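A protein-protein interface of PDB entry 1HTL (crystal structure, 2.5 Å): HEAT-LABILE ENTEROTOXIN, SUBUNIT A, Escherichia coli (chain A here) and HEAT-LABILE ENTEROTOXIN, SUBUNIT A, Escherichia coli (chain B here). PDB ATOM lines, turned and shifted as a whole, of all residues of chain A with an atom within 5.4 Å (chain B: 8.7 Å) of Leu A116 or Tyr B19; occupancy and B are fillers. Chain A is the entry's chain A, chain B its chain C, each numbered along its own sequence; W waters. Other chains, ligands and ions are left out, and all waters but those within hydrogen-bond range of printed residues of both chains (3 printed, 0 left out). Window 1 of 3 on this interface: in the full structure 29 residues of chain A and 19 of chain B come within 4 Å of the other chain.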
ATOM      1  N   TYR A  30      12.227  -8.279  17.317  1.00  0.00           N
ATOM      2  CA  TYR A  30      12.769  -9.641  17.412  1.00  0.00           C
ATOM      3  C   TYR A  30      11.762 -10.789  17.592  1.00  0.00           C
ATOM      4  O   TYR A  30      11.681 -11.668  16.739  1.00  0.00           O
ATOM      5  CB  TYR A  30      13.881  -9.713  18.483  1.00  0.00           C
ATOM      6  CG  TYR A  30      14.768 -10.927  18.359  1.00  0.00           C
ATOM      7  CD1 TYR A  30      15.252 -11.336  17.124  1.00  0.00           C
ATOM      8  CD2 TYR A  30      15.075 -11.701  19.466  1.00  0.00           C
ATOM      9  CE1 TYR A  30      16.014 -12.496  16.994  1.00  0.00           C
ATOM     10  CE2 TYR A  30      15.843 -12.867  19.349  1.00  0.00           C
ATOM     11  CZ  TYR A  30      16.307 -13.252  18.118  1.00  0.00           C
ATOM     12  OH  TYR A  30      17.104 -14.370  18.007  1.00  0.00           O
ATOM     13  N   ILE A  39      13.251 -16.425   5.344  1.00  0.00           N
ATOM     14  CA  ILE A  39      14.622 -16.645   5.806  1.00  0.00           C
ATOM     15  C   ILE A  39      15.331 -17.491   4.753  1.00  0.00           C
ATOM     16  O   ILE A  39      14.823 -18.544   4.348  1.00  0.00           O
ATOM     17  CB  ILE A  39      14.666 -17.398   7.169  1.00  0.00           C
ATOM     18  CG1 ILE A  39      13.851 -16.668   8.227  1.00  0.00           C
ATOM     19  CG2 ILE A  39      16.078 -17.484   7.672  1.00  0.00           C
ATOM     20  CD1 ILE A  39      14.032 -17.244   9.587  1.00  0.00           C
ATOM     21  N   GLY A  58      15.856 -12.374   6.238  1.00  0.00           N
ATOM     22  CA  GLY A  58      15.956 -13.003   7.549  1.00  0.00           C
ATOM     23  C   GLY A  58      17.315 -13.082   8.206  1.00  0.00           C
ATOM     24  O   GLY A  58      17.454 -13.758   9.223  1.00  0.00           O
ATOM     25  N   TYR A  59      18.278 -12.332   7.672  1.00  0.00           N
ATOM     26  CA  TYR A  59      19.657 -12.308   8.151  1.00  0.00           C
ATOM     27  C   TYR A  59      20.271 -10.902   8.238  1.00  0.00           C
ATOM     28  O   TYR A  59      20.054 -10.054   7.360  1.00  0.00           O
ATOM     29  CB  TYR A  59      20.525 -13.133   7.211  1.00  0.00           C
ATOM     30  CG  TYR A  59      20.427 -14.621   7.394  1.00  0.00           C
ATOM     31  CD1 TYR A  59      21.172 -15.267   8.366  1.00  0.00           C
ATOM     32  CD2 TYR A  59      19.633 -15.389   6.563  1.00  0.00           C
ATOM     33  CE1 TYR A  59      21.132 -16.634   8.498  1.00  0.00           C
ATOM     34  CE2 TYR A  59      19.588 -16.760   6.696  1.00  0.00           C
ATOM     35  CZ  TYR A  59      20.335 -17.375   7.659  1.00  0.00           C
ATOM     36  OH  TYR A  59      20.282 -18.730   7.795  1.00  0.00           O
ATOM     37  N   PRO A  92      25.469 -19.164  18.642  1.00  0.00           N
ATOM     38  CA  PRO A  92      25.083 -20.083  17.568  1.00  0.00           C
ATOM     39  C   PRO A  92      24.133 -19.542  16.496  1.00  0.00           C
ATOM     40  O   PRO A  92      23.934 -20.182  15.482  1.00  0.00           O
ATOM     41  CB  PRO A  92      24.469 -21.264  18.331  1.00  0.00           C
ATOM     42  CG  PRO A  92      25.100 -21.164  19.697  1.00  0.00           C
ATOM     43  CD  PRO A  92      25.051 -19.691  19.947  1.00  0.00           C
ATOM     44  N   ASN A  93      23.553 -18.372  16.685  1.00  0.00           N
ATOM     45  CA  ASN A  93      22.635 -17.863  15.667  1.00  0.00           C
ATOM     46  C   ASN A  93      23.392 -17.168  14.569  1.00  0.00           C
ATOM     47  O   ASN A  93      22.796 -16.580  13.685  1.00  0.00           O
ATOM     48  CB  ASN A  93      21.562 -16.930  16.264  1.00  0.00           C
ATOM     49  CG  ASN A  93      22.139 -15.638  16.821  1.00  0.00           C
ATOM     50  OD1 ASN A  93      23.294 -15.581  17.247  1.00  0.00           O
ATOM     51  ND2 ASN A  93      21.327 -14.592  16.824  1.00  0.00           N
ATOM     52  N   MET A  94      24.711 -17.239  14.637  1.00  0.00           N
ATOM     53  CA  MET A  94      25.574 -16.622  13.646  1.00  0.00           C
ATOM     54  C   MET A  94      26.082 -17.741  12.723  1.00  0.00           C
ATOM     55  O   MET A  94      26.358 -18.852  13.195  1.00  0.00           O
ATOM     56  CB  MET A  94      26.793 -15.958  14.330  1.00  0.00           C
ATOM     57  CG  MET A  94      26.509 -14.993  15.490  1.00  0.00           C
ATOM     58  SD  MET A  94      25.447 -13.573  15.098  1.00  0.00           S
ATOM     59  CE  MET A  94      26.320 -12.788  13.716  1.00  0.00           C
ATOM     60  N   PHE A  95      26.258 -17.426  11.437  1.00  0.00           N
ATOM     61  CA  PHE A  95      26.765 -18.370  10.437  1.00  0.00           C
ATOM     62  C   PHE A  95      27.832 -17.715   9.578  1.00  0.00           C
ATOM     63  O   PHE A  95      27.603 -16.648   9.011  1.00  0.00           O
ATOM     64  CB  PHE A  95      25.638 -18.827   9.513  1.00  0.00           C
ATOM     65  CG  PHE A  95      24.742 -19.829  10.130  1.00  0.00           C
ATOM     66  CD1 PHE A  95      25.175 -21.127  10.323  1.00  0.00           C
ATOM     67  CD2 PHE A  95      23.488 -19.474  10.546  1.00  0.00           C
ATOM     68  CE1 PHE A  95      24.359 -22.054  10.931  1.00  0.00           C
ATOM     69  CE2 PHE A  95      22.665 -20.388  11.151  1.00  0.00           C
ATOM     70  CZ  PHE A  95      23.092 -21.683  11.349  1.00  0.00           C
ATOM     71  N   SER A 114      26.734 -13.761   9.031  1.00  0.00           N
ATOM     72  CA  SER A 114      25.314 -13.423   9.048  1.00  0.00           C
ATOM     73  C   SER A 114      24.614 -14.027  10.237  1.00  0.00           C
ATOM     74  O   SER A 114      24.935 -15.133  10.650  1.00  0.00           O
ATOM     75  CB  SER A 114      24.658 -13.930   7.765  1.00  0.00           C
ATOM     76  OG  SER A 114      24.922 -13.048   6.684  1.00  0.00           O
ATOM     77  N   ALA A 115      23.624 -13.322  10.764  1.00  0.00           N
ATOM     78  CA  ALA A 115      22.880 -13.817  11.918  1.00  0.00           C
ATOM     79  C   ALA A 115      21.434 -14.158  11.614  1.00  0.00           C
ATOM     80  O   ALA A 115      20.669 -13.319  11.119  1.00  0.00           O
ATOM     81  CB  ALA A 115      22.949 -12.819  13.073  1.00  0.00           C
ATOM     82  N   LEU A 116      21.041 -15.368  11.997  1.00  0.00           N
ATOM     83  CA  LEU A 116      19.693 -15.863  11.778  1.00  0.00           C
ATOM     84  C   LEU A 116      18.608 -15.181  12.614  1.00  0.00           C
ATOM     85  O   LEU A 116      18.605 -15.290  13.833  1.00  0.00           O
ATOM     86  CB  LEU A 116      19.690 -17.378  12.031  1.00  0.00           C
ATOM     87  CG  LEU A 116      18.486 -18.266  11.712  1.00  0.00           C
ATOM     88  CD1 LEU A 116      17.575 -17.588  10.726  1.00  0.00           C
ATOM     89  CD2 LEU A 116      18.973 -19.602  11.194  1.00  0.00           C
ATOM     90  N   GLY A 117      17.680 -14.504  11.944  1.00  0.00           N
ATOM     91  CA  GLY A 117      16.567 -13.852  12.617  1.00  0.00           C
ATOM     92  C   GLY A 117      16.842 -12.485  13.183  1.00  0.00           C
ATOM     93  O   GLY A 117      15.935 -11.764  13.570  1.00  0.00           O
ATOM     94  N   GLY A 118      18.103 -12.095  13.200  1.00  0.00           N
ATOM     95  CA  GLY A 118      18.438 -10.804  13.744  1.00  0.00           C
ATOM     96  C   GLY A 118      19.349 -11.029  14.930  1.00  0.00           C
ATOM     97  O   GLY A 118      19.794 -12.169  15.148  1.00  0.00           O
ATOM     98  N   ALA A 156      27.851 -20.489  14.999  1.00  0.00           N
ATOM     99  CA  ALA A 156      27.343 -21.793  14.650  1.00  0.00           C
ATOM    100  C   ALA A 156      28.317 -22.413  13.654  1.00  0.00           C
ATOM    101  O   ALA A 156      28.711 -21.772  12.671  1.00  0.00           O
ATOM    102  CB  ALA A 156      25.993 -21.670  14.038  1.00  0.00           C
ATOM    103  N   ASP A 160      26.001 -27.061  10.657  1.00  0.00           N
ATOM    104  CA  ASP A 160      24.628 -26.830  11.111  1.00  0.00           C
ATOM    105  C   ASP A 160      23.903 -25.903  10.143  1.00  0.00           C
ATOM    106  O   ASP A 160      22.676 -25.764  10.193  1.00  0.00           O
ATOM    107  CB  ASP A 160      24.604 -26.219  12.523  1.00  0.00           C
ATOM    108  CG  ASP A 160      25.087 -27.181  13.595  1.00  0.00           C
ATOM    109  OD1 ASP A 160      25.216 -28.390  13.301  1.00  0.00           O
ATOM    110  OD2 ASP A 160      25.338 -26.729  14.737  1.00  0.00           O
ATOM    111  N   ARG A 163      22.275 -27.241   5.587  1.00  0.00           N
ATOM    112  CA  ARG A 163      20.861 -27.477   5.273  1.00  0.00           C
ATOM    113  C   ARG A 163      20.129 -26.142   5.126  1.00  0.00           C
ATOM    114  O   ARG A 163      19.084 -26.051   4.478  1.00  0.00           O
ATOM    115  CB  ARG A 163      20.213 -28.312   6.377  1.00  0.00           C
ATOM    116  CG  ARG A 163      20.397 -27.689   7.733  1.00  0.00           C
ATOM    117  CD  ARG A 163      20.098 -28.615   8.896  1.00  0.00           C
ATOM    118  NE  ARG A 163      20.632 -28.040  10.137  1.00  0.00           N
ATOM    119  CZ  ARG A 163      19.980 -27.189  10.934  1.00  0.00           C
ATOM    120  NH1 ARG A 163      18.738 -26.802  10.648  1.00  0.00           N
ATOM    121  NH2 ARG A 163      20.601 -26.664  11.987  1.00  0.00           N
ATOM    122  N   LEU A 164      20.691 -25.107   5.740  1.00  0.00           N
ATOM    123  CA  LEU A 164      20.118 -23.755   5.691  1.00  0.00           C
ATOM    124  C   LEU A 164      20.727 -22.882   4.591  1.00  0.00           C
ATOM    125  O   LEU A 164      20.311 -21.754   4.380  1.00  0.00           O
ATOM    126  CB  LEU A 164      20.291 -23.081   7.044  1.00  0.00           C
ATOM    127  CG  LEU A 164      19.715 -23.881   8.210  1.00  0.00           C
ATOM    128  CD1 LEU A 164      19.976 -23.174   9.542  1.00  0.00           C
ATOM    129  CD2 LEU A 164      18.246 -24.042   7.981  1.00  0.00           C
ATOM    130  N   THR B  12      13.517 -24.955   3.379  1.00  0.00           N
ATOM    131  CA  THR B  12      14.558 -24.022   3.763  1.00  0.00           C
ATOM    132  C   THR B  12      13.974 -23.052   4.785  1.00  0.00           C
ATOM    133  O   THR B  12      14.404 -23.009   5.935  1.00  0.00           O
ATOM    134  CB  THR B  12      15.057 -23.277   2.510  1.00  0.00           C
ATOM    135  OG1 THR B  12      15.721 -24.212   1.648  1.00  0.00           O
ATOM    136  CG2 THR B  12      16.003 -22.144   2.874  1.00  0.00           C
ATOM    137  N   GLN B  13      12.898 -22.381   4.393  1.00  0.00           N
ATOM    138  CA  GLN B  13      12.243 -21.430   5.270  1.00  0.00           C
ATOM    139  C   GLN B  13      11.777 -22.078   6.572  1.00  0.00           C
ATOM    140  O   GLN B  13      11.698 -21.412   7.600  1.00  0.00           O
ATOM    141  CB  GLN B  13      11.066 -20.771   4.554  1.00  0.00           C
ATOM    142  CG  GLN B  13      11.223 -19.267   4.423  1.00  0.00           C
ATOM    143  CD  GLN B  13      10.123 -18.487   5.151  1.00  0.00           C
ATOM    144  OE1 GLN B  13       9.169 -18.011   4.530  1.00  0.00           O
ATOM    145  NE2 GLN B  13      10.260 -18.341   6.461  1.00  0.00           N
ATOM    146  N   ASN B  14      11.560 -23.388   6.546  1.00  0.00           N
ATOM    147  CA  ASN B  14      11.082 -24.126   7.716  1.00  0.00           C
ATOM    148  C   ASN B  14      12.163 -24.614   8.689  1.00  0.00           C
ATOM    149  O   ASN B  14      11.939 -24.697   9.900  1.00  0.00           O
ATOM    150  CB  ASN B  14      10.229 -25.307   7.257  1.00  0.00           C
ATOM    151  CG  ASN B  14       9.470 -25.954   8.396  1.00  0.00           C
ATOM    152  OD1 ASN B  14       8.818 -25.272   9.193  1.00  0.00           O
ATOM    153  ND2 ASN B  14       9.526 -27.285   8.466  1.00  0.00           N
ATOM    154  N   LEU B  15      13.311 -24.999   8.161  1.00  0.00           N
ATOM    155  CA  LEU B  15      14.397 -25.461   9.007  1.00  0.00           C
ATOM    156  C   LEU B  15      14.994 -24.210   9.609  1.00  0.00           C
ATOM    157  O   LEU B  15      15.465 -24.208  10.738  1.00  0.00           O
ATOM    158  CB  LEU B  15      15.432 -26.205   8.173  1.00  0.00           C
ATOM    159  CG  LEU B  15      14.791 -27.334   7.363  1.00  0.00           C
ATOM    160  CD1 LEU B  15      15.845 -27.987   6.495  1.00  0.00           C
ATOM    161  CD2 LEU B  15      14.157 -28.341   8.305  1.00  0.00           C
ATOM    162  N   SER B  16      14.926 -23.127   8.852  1.00  0.00           N
ATOM    163  CA  SER B  16      15.418 -21.856   9.311  1.00  0.00           C
ATOM    164  C   SER B  16      14.559 -21.346  10.473  1.00  0.00           C
ATOM    165  O   SER B  16      15.082 -21.075  11.545  1.00  0.00           O
ATOM    166  CB  SER B  16      15.427 -20.886   8.143  1.00  0.00           C
ATOM    167  OG  SER B  16      16.287 -21.389   7.136  1.00  0.00           O
ATOM    168  N   THR B  17      13.241 -21.285  10.274  1.00  0.00           N
ATOM    169  CA  THR B  17      12.283 -20.820  11.284  1.00  0.00           C
ATOM    170  C   THR B  17      12.331 -21.628  12.575  1.00  0.00           C
ATOM    171  O   THR B  17      12.148 -21.071  13.662  1.00  0.00           O
ATOM    172  CB  THR B  17      10.825 -20.868  10.768  1.00  0.00           C
ATOM    173  OG1 THR B  17      10.702 -20.121   9.554  1.00  0.00           O
ATOM    174  CG2 THR B  17       9.891 -20.271  11.768  1.00  0.00           C
ATOM    175  N   ILE B  18      12.527 -22.941  12.466  1.00  0.00           N
ATOM    176  CA  ILE B  18      12.597 -23.790  13.654  1.00  0.00           C
ATOM    177  C   ILE B  18      13.945 -23.569  14.345  1.00  0.00           C
ATOM    178  O   ILE B  18      14.100 -23.857  15.535  1.00  0.00           O
ATOM    179  CB  ILE B  18      12.398 -25.279  13.305  1.00  0.00           C
ATOM    180  CG1 ILE B  18      11.006 -25.464  12.704  1.00  0.00           C
ATOM    181  CG2 ILE B  18      12.556 -26.156  14.548  1.00  0.00           C
ATOM    182  CD1 ILE B  18      10.683 -26.894  12.339  1.00  0.00           C
ATOM    183  N   TYR B  19      14.922 -23.085  13.581  1.00  0.00           N
ATOM    184  CA  TYR B  19      16.233 -22.779  14.124  1.00  0.00           C
ATOM    185  C   TYR B  19      16.039 -21.447  14.872  1.00  0.00           C
ATOM    186  O   TYR B  19      16.533 -21.260  15.978  1.00  0.00           O
ATOM    187  CB  TYR B  19      17.271 -22.639  13.000  1.00  0.00           C
ATOM    188  CG  TYR B  19      18.693 -22.616  13.502  1.00  0.00           C
ATOM    189  CD1 TYR B  19      19.157 -21.574  14.302  1.00  0.00           C
ATOM    190  CD2 TYR B  19      19.565 -23.652  13.217  1.00  0.00           C
ATOM    191  CE1 TYR B  19      20.451 -21.570  14.807  1.00  0.00           C
ATOM    192  CE2 TYR B  19      20.861 -23.651  13.717  1.00  0.00           C
ATOM    193  CZ  TYR B  19      21.291 -22.601  14.513  1.00  0.00           C
ATOM    194  OH  TYR B  19      22.577 -22.599  14.996  1.00  0.00           O
ATOM    195  N   LEU B  20      15.266 -20.547  14.279  1.00  0.00           N
ATOM    196  CA  LEU B  20      14.983 -19.275  14.904  1.00  0.00           C
ATOM    197  C   LEU B  20      14.228 -19.480  16.213  1.00  0.00           C
ATOM    198  O   LEU B  20      14.761 -19.209  17.275  1.00  0.00           O
ATOM    199  CB  LEU B  20      14.154 -18.379  13.980  1.00  0.00           C
ATOM    200  CG  LEU B  20      13.804 -17.041  14.644  1.00  0.00           C
ATOM    201  CD1 LEU B  20      15.085 -16.331  15.050  1.00  0.00           C
ATOM    202  CD2 LEU B  20      12.979 -16.152  13.716  1.00  0.00           C
ATOM    203  N   ARG B  21      13.004 -19.989  16.122  1.00  0.00           N
ATOM    204  CA  ARG B  21      12.129 -20.215  17.271  1.00  0.00           C
ATOM    205  C   ARG B  21      12.744 -20.889  18.480  1.00  0.00           C
ATOM    206  O   ARG B  21      12.284 -20.682  19.605  1.00  0.00           O
ATOM    207  CB  ARG B  21      10.882 -20.967  16.829  1.00  0.00           C
ATOM    208  CG  ARG B  21      10.125 -20.212  15.762  1.00  0.00           C
ATOM    209  CD  ARG B  21       9.537 -18.947  16.332  1.00  0.00           C
ATOM    210  NE  ARG B  21       9.466 -17.851  15.369  1.00  0.00           N
ATOM    211  CZ  ARG B  21       8.436 -17.625  14.560  1.00  0.00           C
ATOM    212  NH1 ARG B  21       7.373 -18.444  14.575  1.00  0.00           N
ATOM    213  NH2 ARG B  21       8.431 -16.521  13.805  1.00  0.00           N
ATOM    214  N   GLU B  22      13.736 -21.739  18.257  1.00  0.00           N
ATOM    215  CA  GLU B  22      14.391 -22.409  19.371  1.00  0.00           C
ATOM    216  C   GLU B  22      15.438 -21.497  19.980  1.00  0.00           C
ATOM    217  O   GLU B  22      15.654 -21.537  21.184  1.00  0.00           O
ATOM    218  CB  GLU B  22      15.013 -23.744  18.956  1.00  0.00           C
ATOM    219  CG  GLU B  22      14.032 -24.913  19.002  1.00  0.00           C
ATOM    220  CD  GLU B  22      14.681 -26.260  18.706  1.00  0.00           C
ATOM    221  OE1 GLU B  22      15.743 -26.584  19.309  1.00  0.00           O
ATOM    222  OE2 GLU B  22      14.106 -27.001  17.873  1.00  0.00           O
ATOM    223  N   TYR B  23      16.093 -20.681  19.153  1.00  0.00           N
ATOM    224  CA  TYR B  23      17.083 -19.730  19.652  1.00  0.00           C
ATOM    225  C   TYR B  23      16.371 -18.595  20.417  1.00  0.00           C
ATOM    226  O   TYR B  23      16.854 -18.157  21.459  1.00  0.00           O
ATOM    227  CB  TYR B  23      17.957 -19.192  18.522  1.00  0.00           C
ATOM    228  CG  TYR B  23      19.047 -18.298  19.017  1.00  0.00           C
ATOM    229  CD1 TYR B  23      20.196 -18.824  19.590  1.00  0.00           C
ATOM    230  CD2 TYR B  23      18.924 -16.913  18.932  1.00  0.00           C
ATOM    231  CE1 TYR B  23      21.193 -17.995  20.064  1.00  0.00           C
ATOM    232  CE2 TYR B  23      19.911 -16.084  19.400  1.00  0.00           C
ATOM    233  CZ  TYR B  23      21.043 -16.620  19.964  1.00  0.00           C
ATOM    234  OH  TYR B  23      22.038 -15.770  20.400  1.00  0.00           O
ATOM    235  N   GLN B  24      15.183 -18.208  19.945  1.00  0.00           N
ATOM    236  CA  GLN B  24      14.344 -17.174  20.570  1.00  0.00           C
ATOM    237  C   GLN B  24      13.848 -17.602  21.943  1.00  0.00           C
ATOM    238  O   GLN B  24      13.388 -16.769  22.735  1.00  0.00           O
ATOM    239  CB  GLN B  24      13.140 -16.829  19.704  1.00  0.00           C
ATOM    240  CG  GLN B  24      13.469 -15.973  18.509  1.00  0.00           C
ATOM    241  CD  GLN B  24      12.234 -15.476  17.795  1.00  0.00           C
ATOM    242  OE1 GLN B  24      11.167 -16.060  17.929  1.00  0.00           O
ATOM    243  NE2 GLN B  24      12.377 -14.422  17.008  1.00  0.00           N
ATOM    244  N   SER B  25      13.927 -18.907  22.206  1.00  0.00           N
ATOM    245  CA  SER B  25      13.553 -19.487  23.499  1.00  0.00           C
ATOM    246  C   SER B  25      14.782 -19.478  24.454  1.00  0.00           C
ATOM    247  O   SER B  25      14.632 -19.290  25.663  1.00  0.00           O
ATOM    248  CB  SER B  25      13.010 -20.901  23.317  1.00  0.00           C
ATOM    249  OG  SER B  25      12.244 -21.259  24.437  1.00  0.00           O
ATOM    250  N   LYS B  26      15.992 -19.658  23.910  1.00  0.00           N
ATOM    251  CA  LYS B  26      17.206 -19.594  24.734  1.00  0.00           C
ATOM    252  C   LYS B  26      17.197 -18.174  25.279  1.00  0.00           C
ATOM    253  O   LYS B  26      17.212 -17.947  26.487  1.00  0.00           O
ATOM    254  CB  LYS B  26      18.488 -19.753  23.900  1.00  0.00           C
ATOM    255  CG  LYS B  26      18.779 -21.128  23.343  1.00  0.00           C
ATOM    256  CD  LYS B  26      18.563 -22.226  24.355  1.00  0.00           C
ATOM    257  CE  LYS B  26      19.304 -23.478  23.939  1.00  0.00           C
ATOM    258  NZ  LYS B  26      18.862 -24.666  24.735  1.00  0.00           N
HETATM  259  O   HOH W   1      16.128 -26.581  11.621  1.00  0.00           O
HETATM  260  O   HOH W   2      10.643 -13.981  14.635  1.00  0.00           O
HETATM  261  O   HOH W   3      18.488 -20.365   5.963  1.00  0.00           O
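OD1 of Asn A93 sits at hydrogen-bond distance from OH of Tyr B23.
The backbone carbonyl oxygen (O) of Tyr A30 sits at hydrogen-bond distance from the side-chain amide nitrogen (NE2) of Gln B24 (2.9 Å).
The backbone carbonyl oxygen (O) of Pro A92 is in hydrogen-bond range of the side-chain hydroxyl (OH) of Tyr B19 (2.8 Å).
The side-chain hydroxyl of Ser B16 is in hydrogen-bond range of the backbone carbonyl oxygen of Thr B12, 2.8 Å away.
The backbone carbonyl oxygen of Asp A160 sits at hydrogen-bond distance from the guanidinium group of Arg A163, at 2.9 Å.
The backbone carbonyl oxygen (O) of Gln B13 lies within hydrogen-bond range of the side-chain hydroxyl (OG1) of Thr B17, at 2.5 Å.
The side-chain amide nitrogen (ND2) of Asn A93 is in hydrogen-bond range of the backbone carbonyl oxygen (O) of Gly A118, at 3.3 Å.
O of Gly A58 sits at hydrogen-bond distance from N of Gly A117 (2.8 Å).
OD1 of Asn A93 lies close to SD of Met A94 (3.6 Å).
Tyr B23 touches Tyr A30 (CD2 to OH, 3.3 Å).
Gln B13 touches Ile A39 (CG to N, 3.6 Å).
Ser B16 touches Ile A39.
Leu A116 touches Tyr B19 (CD2 to CD1, 3.7 Å).
Gly A117 touches Leu B20.
Tyr B19 touches Ala A156 (OH to CB, 3.7 Å).
Arg A163 touches Tyr B19.
CD2 of Leu A164 touches CB of Leu B15 (3.6 Å).
Ser B16 touches Leu A164 (OG to CD2, 3.4 Å).
CD1 of Leu A164 touches CD2 of Tyr B19 (3.7 Å).
Tyr B19 touches just these residues of chain A: Pro A92, Phe A95, Leu A116, Ala A156, Arg A163 and Leu A164.
No residue of chain B comes within 4 Å of Ala A115.
Of chain B, only Leu B20 (3.8 Å) comes within 4 Å of Gly A117.
No residue of chain B comes within 4 Å of Gly A118.
Of the printed residues of chain B, Ala A156 touches Tyr B19 (3.7 Å).
Printed residues of chain B within 4 Å of Asn A93: Tyr B23.
Printed residues of chain A within 4 Å of Tyr B23: Tyr A30 and Asn A93.
Printed residues of chain B within 4 Å of Tyr A30: Tyr B23 and Gln B24.
Of the printed residues of chain A, Gln B24 touches Tyr A30.
Asn B14 touches none of the printed residues of chain A.
The nearest residue of chain B that does not touch Leu A116 is Ser B16 (4.2 Å).
The nearest residue of chain A that does not touch Tyr B19 is Asn A93 (4.4 Å).
Of the 17 printed residues of chain A, 10 touch a printed residue of chain B.
Hydrophobic or aromatic side chains of chain A within 4 Å of the printed part of chain B: Tyr A30, Ile A39, Phe A95, Leu A116, Ala A156 and Leu A164.
Along chain B the printed residues that touch a printed residue of chain A span positions 13 to 24.
Among the printed residues, 15 pairs touch across the chains.
Among the printed residues, no Asp or Glu carboxylate lies within 4 Å of a Lys or Arg side-chain nitrogen of the other chain.
Water W1 lies within hydrogen-bond range of O of Leu B15 (2.6 Å) and NH1 of Arg A163 (2.8 Å).
Water W3 lies within hydrogen-bond range of OG of Ser B16 (2.7 Å), O of Leu A164 (2.8 Å) and OH of Tyr A59 (3.0 Å).
Water W2 lies within hydrogen-bond range of NE2 of Gln B24 (3.0 Å), O of Tyr A30 (3.3 Å) and NH2 of Arg B21 (3.5 Å).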
